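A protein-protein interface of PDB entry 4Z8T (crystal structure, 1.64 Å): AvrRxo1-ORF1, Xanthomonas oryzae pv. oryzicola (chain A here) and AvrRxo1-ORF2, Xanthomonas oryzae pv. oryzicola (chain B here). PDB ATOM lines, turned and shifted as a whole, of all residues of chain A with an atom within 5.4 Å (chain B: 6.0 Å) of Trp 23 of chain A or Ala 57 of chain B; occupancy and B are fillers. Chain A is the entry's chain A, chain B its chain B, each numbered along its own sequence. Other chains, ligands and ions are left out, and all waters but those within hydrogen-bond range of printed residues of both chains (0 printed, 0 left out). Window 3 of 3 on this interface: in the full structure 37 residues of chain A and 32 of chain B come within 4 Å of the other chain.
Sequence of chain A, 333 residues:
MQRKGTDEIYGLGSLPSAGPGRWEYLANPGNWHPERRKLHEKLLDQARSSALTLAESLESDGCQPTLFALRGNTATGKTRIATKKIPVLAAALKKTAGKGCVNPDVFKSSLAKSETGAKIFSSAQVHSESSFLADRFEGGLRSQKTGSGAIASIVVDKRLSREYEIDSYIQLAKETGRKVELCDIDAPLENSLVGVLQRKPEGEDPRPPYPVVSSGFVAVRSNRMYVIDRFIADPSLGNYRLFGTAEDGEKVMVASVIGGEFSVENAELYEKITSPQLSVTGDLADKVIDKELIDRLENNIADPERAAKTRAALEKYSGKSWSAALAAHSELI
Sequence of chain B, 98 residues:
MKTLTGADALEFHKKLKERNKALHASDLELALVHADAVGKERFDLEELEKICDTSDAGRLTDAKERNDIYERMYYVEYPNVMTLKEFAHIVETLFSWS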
ATOM      1  N   ALA A  18       3.756 -18.085  22.458  1.00  0.00           N
ATOM      2  CA  ALA A  18       5.116 -17.605  22.242  1.00  0.00           C
ATOM      3  C   ALA A  18       6.103 -17.499  23.425  1.00  0.00           C
ATOM      4  O   ALA A  18       7.289 -17.257  23.210  1.00  0.00           O
ATOM      5  CB  ALA A  18       5.123 -16.359  21.413  1.00  0.00           C
ATOM      6  N   GLY A  19       5.634 -17.649  24.654  1.00  0.00           N
ATOM      7  CA  GLY A  19       6.533 -17.653  25.788  1.00  0.00           C
ATOM      8  C   GLY A  19       7.202 -19.010  25.764  1.00  0.00           C
ATOM      9  O   GLY A  19       7.005 -19.754  24.830  1.00  0.00           O
ATOM     10  N   PRO A  20       8.005 -19.360  26.747  1.00  0.00           N
ATOM     11  CA  PRO A  20       8.693 -20.637  26.645  1.00  0.00           C
ATOM     12  C   PRO A  20       7.612 -21.694  26.545  1.00  0.00           C
ATOM     13  O   PRO A  20       6.452 -21.454  26.813  1.00  0.00           O
ATOM     14  CB  PRO A  20       9.428 -20.745  27.961  1.00  0.00           C
ATOM     15  CG  PRO A  20       8.607 -20.053  28.858  1.00  0.00           C
ATOM     16  CD  PRO A  20       7.975 -18.910  28.131  1.00  0.00           C
ATOM     17  N   GLY A  21       8.021 -22.875  26.099  1.00  0.00           N
ATOM     18  CA  GLY A  21       7.101 -23.884  25.614  1.00  0.00           C
ATOM     19  C   GLY A  21       7.197 -23.795  24.105  1.00  0.00           C
ATOM     20  O   GLY A  21       7.201 -24.802  23.397  1.00  0.00           O
ATOM     21  N   ARG A  22       7.289 -22.559  23.622  1.00  0.00           N
ATOM     22  CA  ARG A  22       7.624 -22.268  22.245  1.00  0.00           C
ATOM     23  C   ARG A  22       9.132 -22.404  22.060  1.00  0.00           C
ATOM     24  O   ARG A  22       9.610 -22.515  20.932  1.00  0.00           O
ATOM     25  CB  ARG A  22       7.170 -20.858  21.867  1.00  0.00           C
ATOM     26  CG  ARG A  22       8.150 -20.107  20.981  1.00  0.00           C
ATOM     27  CD  ARG A  22       7.463 -19.549  19.746  1.00  0.00           C
ATOM     28  NE  ARG A  22       7.592 -18.097  19.655  1.00  0.00           N
ATOM     29  CZ  ARG A  22       6.851 -17.329  18.863  1.00  0.00           C
ATOM     30  NH1 ARG A  22       7.038 -16.017  18.845  1.00  0.00           N
ATOM     31  NH2 ARG A  22       5.924 -17.874  18.087  1.00  0.00           N
ATOM     32  N   TRP A  23       9.888 -22.400  23.161  1.00  0.00           N
ATOM     33  CA  TRP A  23      11.328 -22.570  23.032  1.00  0.00           C
ATOM     34  C   TRP A  23      11.749 -24.036  22.878  1.00  0.00           C
ATOM     35  O   TRP A  23      12.371 -24.366  21.880  1.00  0.00           O
ATOM     36  CB  TRP A  23      12.098 -21.786  24.108  1.00  0.00           C
ATOM     37  CG  TRP A  23      11.953 -20.295  23.883  1.00  0.00           C
ATOM     38  CD1 TRP A  23      10.909 -19.508  24.276  1.00  0.00           C
ATOM     39  CD2 TRP A  23      12.857 -19.432  23.170  1.00  0.00           C
ATOM     40  NE1 TRP A  23      11.111 -18.209  23.869  1.00  0.00           N
ATOM     41  CE2 TRP A  23      12.298 -18.135  23.189  1.00  0.00           C
ATOM     42  CE3 TRP A  23      14.085 -19.627  22.528  1.00  0.00           C
ATOM     43  CZ2 TRP A  23      12.927 -17.040  22.589  1.00  0.00           C
ATOM     44  CZ3 TRP A  23      14.707 -18.537  21.932  1.00  0.00           C
ATOM     45  CH2 TRP A  23      14.128 -17.262  21.969  1.00  0.00           C
ATOM     46  N   GLU A  24      11.371 -24.911  23.810  1.00  0.00           N
ATOM     47  CA  GLU A  24      11.648 -26.349  23.675  1.00  0.00           C
ATOM     48  C   GLU A  24      11.140 -26.933  22.360  1.00  0.00           C
ATOM     49  O   GLU A  24      11.773 -27.812  21.773  1.00  0.00           O
ATOM     50  CB  GLU A  24      11.022 -27.135  24.823  1.00  0.00           C
ATOM     51  CG  GLU A  24      11.837 -27.165  26.096  1.00  0.00           C
ATOM     52  CD  GLU A  24      10.982 -27.512  27.295  1.00  0.00           C
ATOM     53  OE1 GLU A  24       9.824 -27.043  27.344  1.00  0.00           O
ATOM     54  OE2 GLU A  24      11.456 -28.258  28.176  1.00  0.00           O
ATOM     55  N   TYR A  25       9.980 -26.454  21.920  1.00  0.00           N
ATOM     56  CA  TYR A  25       9.418 -26.856  20.641  1.00  0.00           C
ATOM     57  C   TYR A  25      10.407 -26.508  19.546  1.00  0.00           C
ATOM     58  O   TYR A  25      10.774 -27.353  18.729  1.00  0.00           O
ATOM     59  CB  TYR A  25       8.104 -26.120  20.389  1.00  0.00           C
ATOM     60  CG  TYR A  25       7.333 -26.618  19.189  1.00  0.00           C
ATOM     61  CD1 TYR A  25       6.394 -27.632  19.321  1.00  0.00           C
ATOM     62  CD2 TYR A  25       7.534 -26.072  17.926  1.00  0.00           C
ATOM     63  CE1 TYR A  25       5.679 -28.093  18.234  1.00  0.00           C
ATOM     64  CE2 TYR A  25       6.823 -26.527  16.829  1.00  0.00           C
ATOM     65  CZ  TYR A  25       5.897 -27.538  16.990  1.00  0.00           C
ATOM     66  OH  TYR A  25       5.186 -27.998  15.906  1.00  0.00           O
ATOM     67  N   LEU A  26      10.840 -25.252  19.547  1.00  0.00           N
ATOM     68  CA  LEU A  26      11.799 -24.771  18.564  1.00  0.00           C
ATOM     69  C   LEU A  26      13.242 -25.093  18.948  1.00  0.00           C
ATOM     70  O   LEU A  26      14.120 -25.101  18.089  1.00  0.00           O
ATOM     71  CB  LEU A  26      11.611 -23.274  18.309  1.00  0.00           C
ATOM     72  CG  LEU A  26      10.323 -22.966  17.539  1.00  0.00           C
ATOM     73  CD1 LEU A  26      10.182 -21.488  17.267  1.00  0.00           C
ATOM     74  CD2 LEU A  26      10.269 -23.749  16.235  1.00  0.00           C
ATOM     75  N   ALA A  27      13.481 -25.378  20.226  1.00  0.00           N
ATOM     76  CA  ALA A  27      14.808 -25.820  20.661  1.00  0.00           C
ATOM     77  C   ALA A  27      15.129 -27.168  20.041  1.00  0.00           C
ATOM     78  O   ALA A  27      16.293 -27.520  19.887  1.00  0.00           O
ATOM     79  CB  ALA A  27      14.910 -25.891  22.181  1.00  0.00           C
ATOM     80  N   ASN A  28      14.085 -27.920  19.704  1.00  0.00           N
ATOM     81  CA  ASN A  28      14.224 -29.146  18.932  1.00  0.00           C
ATOM     82  C   ASN A  28      14.484 -28.789  17.482  1.00  0.00           C
ATOM     83  O   ASN A  28      13.581 -28.320  16.784  1.00  0.00           O
ATOM     84  CB  ASN A  28      12.946 -29.980  19.039  1.00  0.00           C
ATOM     85  CG  ASN A  28      12.856 -31.065  17.975  1.00  0.00           C
ATOM     86  OD1 ASN A  28      13.860 -31.669  17.594  1.00  0.00           O
ATOM     87  ND2 ASN A  28      11.644 -31.313  17.489  1.00  0.00           N
ATOM     88  N   SER A 128      14.531 -14.019  17.711  1.00  0.00           N
ATOM     89  CA  SER A 128      14.231 -15.268  18.409  1.00  0.00           C
ATOM     90  C   SER A 128      15.045 -16.415  17.836  1.00  0.00           C
ATOM     91  O   SER A 128      15.653 -17.192  18.570  1.00  0.00           O
ATOM     92  CB  SER A 128      12.741 -15.595  18.325  1.00  0.00           C
ATOM     93  OG  SER A 128      11.993 -14.679  19.101  1.00  0.00           O
ATOM     94  N   SER A 131      18.640 -16.151  18.806  1.00  0.00           N
ATOM     95  CA  SER A 131      18.823 -16.479  20.222  1.00  0.00           C
ATOM     96  C   SER A 131      18.846 -17.994  20.390  1.00  0.00           C
ATOM     97  O   SER A 131      19.682 -18.540  21.115  1.00  0.00           O
ATOM     98  CB  SER A 131      17.723 -15.837  21.072  1.00  0.00           C
ATOM     99  OG  SER A 131      17.925 -16.108  22.449  1.00  0.00           O
ATOM    100  N   PHE A 132      17.944 -18.669  19.687  1.00  0.00           N
ATOM    101  CA  PHE A 132      17.940 -20.124  19.652  1.00  0.00           C
ATOM    102  C   PHE A 132      19.277 -20.684  19.163  1.00  0.00           C
ATOM    103  O   PHE A 132      19.823 -21.621  19.751  1.00  0.00           O
ATOM    104  CB  PHE A 132      16.782 -20.615  18.783  1.00  0.00           C
ATOM    105  CG  PHE A 132      17.004 -21.963  18.184  1.00  0.00           C
ATOM    106  CD1 PHE A 132      16.793 -23.112  18.926  1.00  0.00           C
ATOM    107  CD2 PHE A 132      17.403 -22.084  16.861  1.00  0.00           C
ATOM    108  CE1 PHE A 132      16.995 -24.361  18.365  1.00  0.00           C
ATOM    109  CE2 PHE A 132      17.611 -23.331  16.298  1.00  0.00           C
ATOM    110  CZ  PHE A 132      17.402 -24.470  17.055  1.00  0.00           C
ATOM    111  N   ASP A 135      22.023 -20.246  21.782  1.00  0.00           N
ATOM    112  CA  ASP A 135      21.904 -21.178  22.896  1.00  0.00           C
ATOM    113  C   ASP A 135      22.394 -22.561  22.508  1.00  0.00           C
ATOM    114  O   ASP A 135      23.017 -23.264  23.310  1.00  0.00           O
ATOM    115  CB  ASP A 135      20.460 -21.235  23.390  1.00  0.00           C
ATOM    116  CG  ASP A 135      20.038 -19.963  24.071  1.00  0.00           C
ATOM    117  OD1 ASP A 135      20.925 -19.208  24.524  1.00  0.00           O
ATOM    118  OD2 ASP A 135      18.815 -19.719  24.165  1.00  0.00           O
ATOM    119  N   ASP B  53       5.836 -12.564  27.624  1.00  0.00           N
ATOM    120  CA  ASP B  53       6.749 -13.507  28.248  1.00  0.00           C
ATOM    121  C   ASP B  53       7.782 -12.784  29.100  1.00  0.00           C
ATOM    122  O   ASP B  53       8.560 -11.977  28.588  1.00  0.00           O
ATOM    123  CB  ASP B  53       7.464 -14.318  27.169  1.00  0.00           C
ATOM    124  CG  ASP B  53       8.425 -15.336  27.743  1.00  0.00           C
ATOM    125  OD1 ASP B  53       8.220 -15.772  28.894  1.00  0.00           O
ATOM    126  OD2 ASP B  53       9.376 -15.713  27.030  1.00  0.00           O
ATOM    127  N   THR B  54       7.790 -13.086  30.396  1.00  0.00           N
ATOM    128  CA  THR B  54       8.754 -12.515  31.328  1.00  0.00           C
ATOM    129  C   THR B  54       9.841 -13.524  31.675  1.00  0.00           C
ATOM    130  O   THR B  54      10.691 -13.271  32.533  1.00  0.00           O
ATOM    131  CB  THR B  54       8.074 -12.087  32.638  1.00  0.00           C
ATOM    132  OG1 THR B  54       7.367 -13.201  33.199  1.00  0.00           O
ATOM    133  CG2 THR B  54       7.107 -10.938  32.388  1.00  0.00           C
ATOM    134  N   SER B  55       9.812 -14.667  31.000  1.00  0.00           N
ATOM    135  CA  SER B  55      10.654 -15.791  31.383  1.00  0.00           C
ATOM    136  C   SER B  55      12.098 -15.679  30.900  1.00  0.00           C
ATOM    137  O   SER B  55      12.988 -16.314  31.469  1.00  0.00           O
ATOM    138  CB  SER B  55      10.038 -17.096  30.880  1.00  0.00           C
ATOM    139  OG  SER B  55      10.611 -18.212  31.526  1.00  0.00           O
ATOM    140  N   ASP B  56      12.322 -14.871  29.863  1.00  0.00           N
ATOM    141  CA  ASP B  56      13.603 -14.854  29.152  1.00  0.00           C
ATOM    142  C   ASP B  56      13.924 -16.288  28.717  1.00  0.00           C
ATOM    143  O   ASP B  56      15.052 -16.766  28.859  1.00  0.00           O
ATOM    144  CB  ASP B  56      14.717 -14.252  30.024  1.00  0.00           C
ATOM    145  CG  ASP B  56      15.999 -13.987  29.249  1.00  0.00           C
ATOM    146  OD1 ASP B  56      15.954 -13.941  27.998  1.00  0.00           O
ATOM    147  OD2 ASP B  56      17.056 -13.819  29.896  1.00  0.00           O
ATOM    148  N   ALA B  57      12.891 -16.958  28.206  1.00  0.00           N
ATOM    149  CA  ALA B  57      12.950 -18.346  27.742  1.00  0.00           C
ATOM    150  C   ALA B  57      13.311 -19.370  28.819  1.00  0.00           C
ATOM    151  O   ALA B  57      14.021 -20.339  28.546  1.00  0.00           O
ATOM    152  CB  ALA B  57      13.889 -18.475  26.544  1.00  0.00           C
ATOM    153  N   GLY B  58      12.810 -19.169  30.034  1.00  0.00           N
ATOM    154  CA  GLY B  58      13.000 -20.145  31.093  1.00  0.00           C
ATOM    155  C   GLY B  58      14.310 -20.030  31.852  1.00  0.00           C
ATOM    156  O   GLY B  58      14.639 -20.901  32.660  1.00  0.00           O
ATOM    157  N   ARG B  59      15.063 -18.964  31.592  1.00  0.00           N
ATOM    158  CA  ARG B  59      16.300 -18.701  32.324  1.00  0.00           C
ATOM    159  C   ARG B  59      15.973 -18.079  33.663  1.00  0.00           C
ATOM    160  O   ARG B  59      16.640 -18.330  34.669  1.00  0.00           O
ATOM    161  CB  ARG B  59      17.170 -17.716  31.554  1.00  0.00           C
ATOM    162  CG  ARG B  59      17.847 -18.277  30.340  1.00  0.00           C
ATOM    163  CD  ARG B  59      18.529 -17.159  29.578  1.00  0.00           C
ATOM    164  NE  ARG B  59      19.034 -17.626  28.295  1.00  0.00           N
ATOM    165  CZ  ARG B  59      18.261 -17.885  27.248  1.00  0.00           C
ATOM    166  NH1 ARG B  59      16.948 -17.728  27.337  1.00  0.00           N
ATOM    167  NH2 ARG B  59      18.797 -18.306  26.116  1.00  0.00           N
ATOM    168  N   LEU B  60      14.945 -17.240  33.648  1.00  0.00           N
ATOM    169  CA  LEU B  60      14.500 -16.533  34.835  1.00  0.00           C
ATOM    170  C   LEU B  60      13.342 -17.307  35.443  1.00  0.00           C
ATOM    171  O   LEU B  60      12.211 -17.228  34.962  1.00  0.00           O
ATOM    172  CB  LEU B  60      14.067 -15.116  34.458  1.00  0.00           C
ATOM    173  CG  LEU B  60      13.688 -14.148  35.576  1.00  0.00           C
ATOM    174  CD1 LEU B  60      14.700 -14.209  36.707  1.00  0.00           C
ATOM    175  CD2 LEU B  60      13.580 -12.736  35.013  1.00  0.00           C
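Ala 57 of chain B touches one residue of chain A.
Printed residues of chain A within 4 Å of Ser 55 of chain B: Pro 20.
Of the printed residues of chain A, Asp 53 of chain B touches Gly 19 (3.6 Å) and Pro 20 (3.2 Å).
Of the printed residues of chain B, Asp 135 of chain A touches Arg 59.
Asp 56 of chain B touches none of the printed residues of chain A.
The nearest residue of chain B that does not touch Trp 23 of chain A is Asp 53 of chain B (4.4 Å).
The nearest residue of chain A that does not touch Ala 57 of chain B is Pro 20 of chain A (4.2 Å).
The nearest printed residue of chain A that does not touch Arg 59 of chain B is Ser 131 of chain A (4.4 Å).
The backbone NH (N) of Ser 55 of chain B lies within hydrogen-bond range of the side-chain carboxylate (OD1) of Asp 53 of chain B (2.9 Å).
The side-chain hydroxyl (OG) of Ser 55 of chain B sits at hydrogen-bond distance from the backbone NH (N) of Gly 58 of chain B (2.8 Å).
The backbone NH (N) of Leu 60 of chain B lies within hydrogen-bond range of the backbone carbonyl oxygen (O) of Ser 55 of chain B (3.1 Å).
NH1 of Arg 59 of chain B is in salt-bridge range of OD1 of Asp 56 of chain B.
Among the printed residues, pairs that only touch across the chains: Gly 19 of chain A with Asp 53 of chain B (3.6 Å), Pro 20 of chain A with Asp 53 of chain B (3.2 Å), Pro 20 of chain A with Ser 55 of chain B (3.8 Å) and Trp 23 of chain A with Ala 57 of chain B (3.7 Å).
Of the 15 printed residues of chain A, 4 touch a printed residue of chain B.
Hydrophobic or aromatic side chains of chain A within 4 Å of the printed part of chain B: Pro 20 and Trp 23.
Of the 8 printed residues of chain B, 4 touch a printed residue of chain A.
Hydrophobic or aromatic side chains of chain B that line the printed part of chain A: Ala 57.
Among the printed residues, 5 pairs touch across the chains.
The side-chain carboxylate (OD2) of Asp 135 of chain A is in salt-bridge range of the guanidinium group (NH2) of Arg 59 of chain B (2.4 Å).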
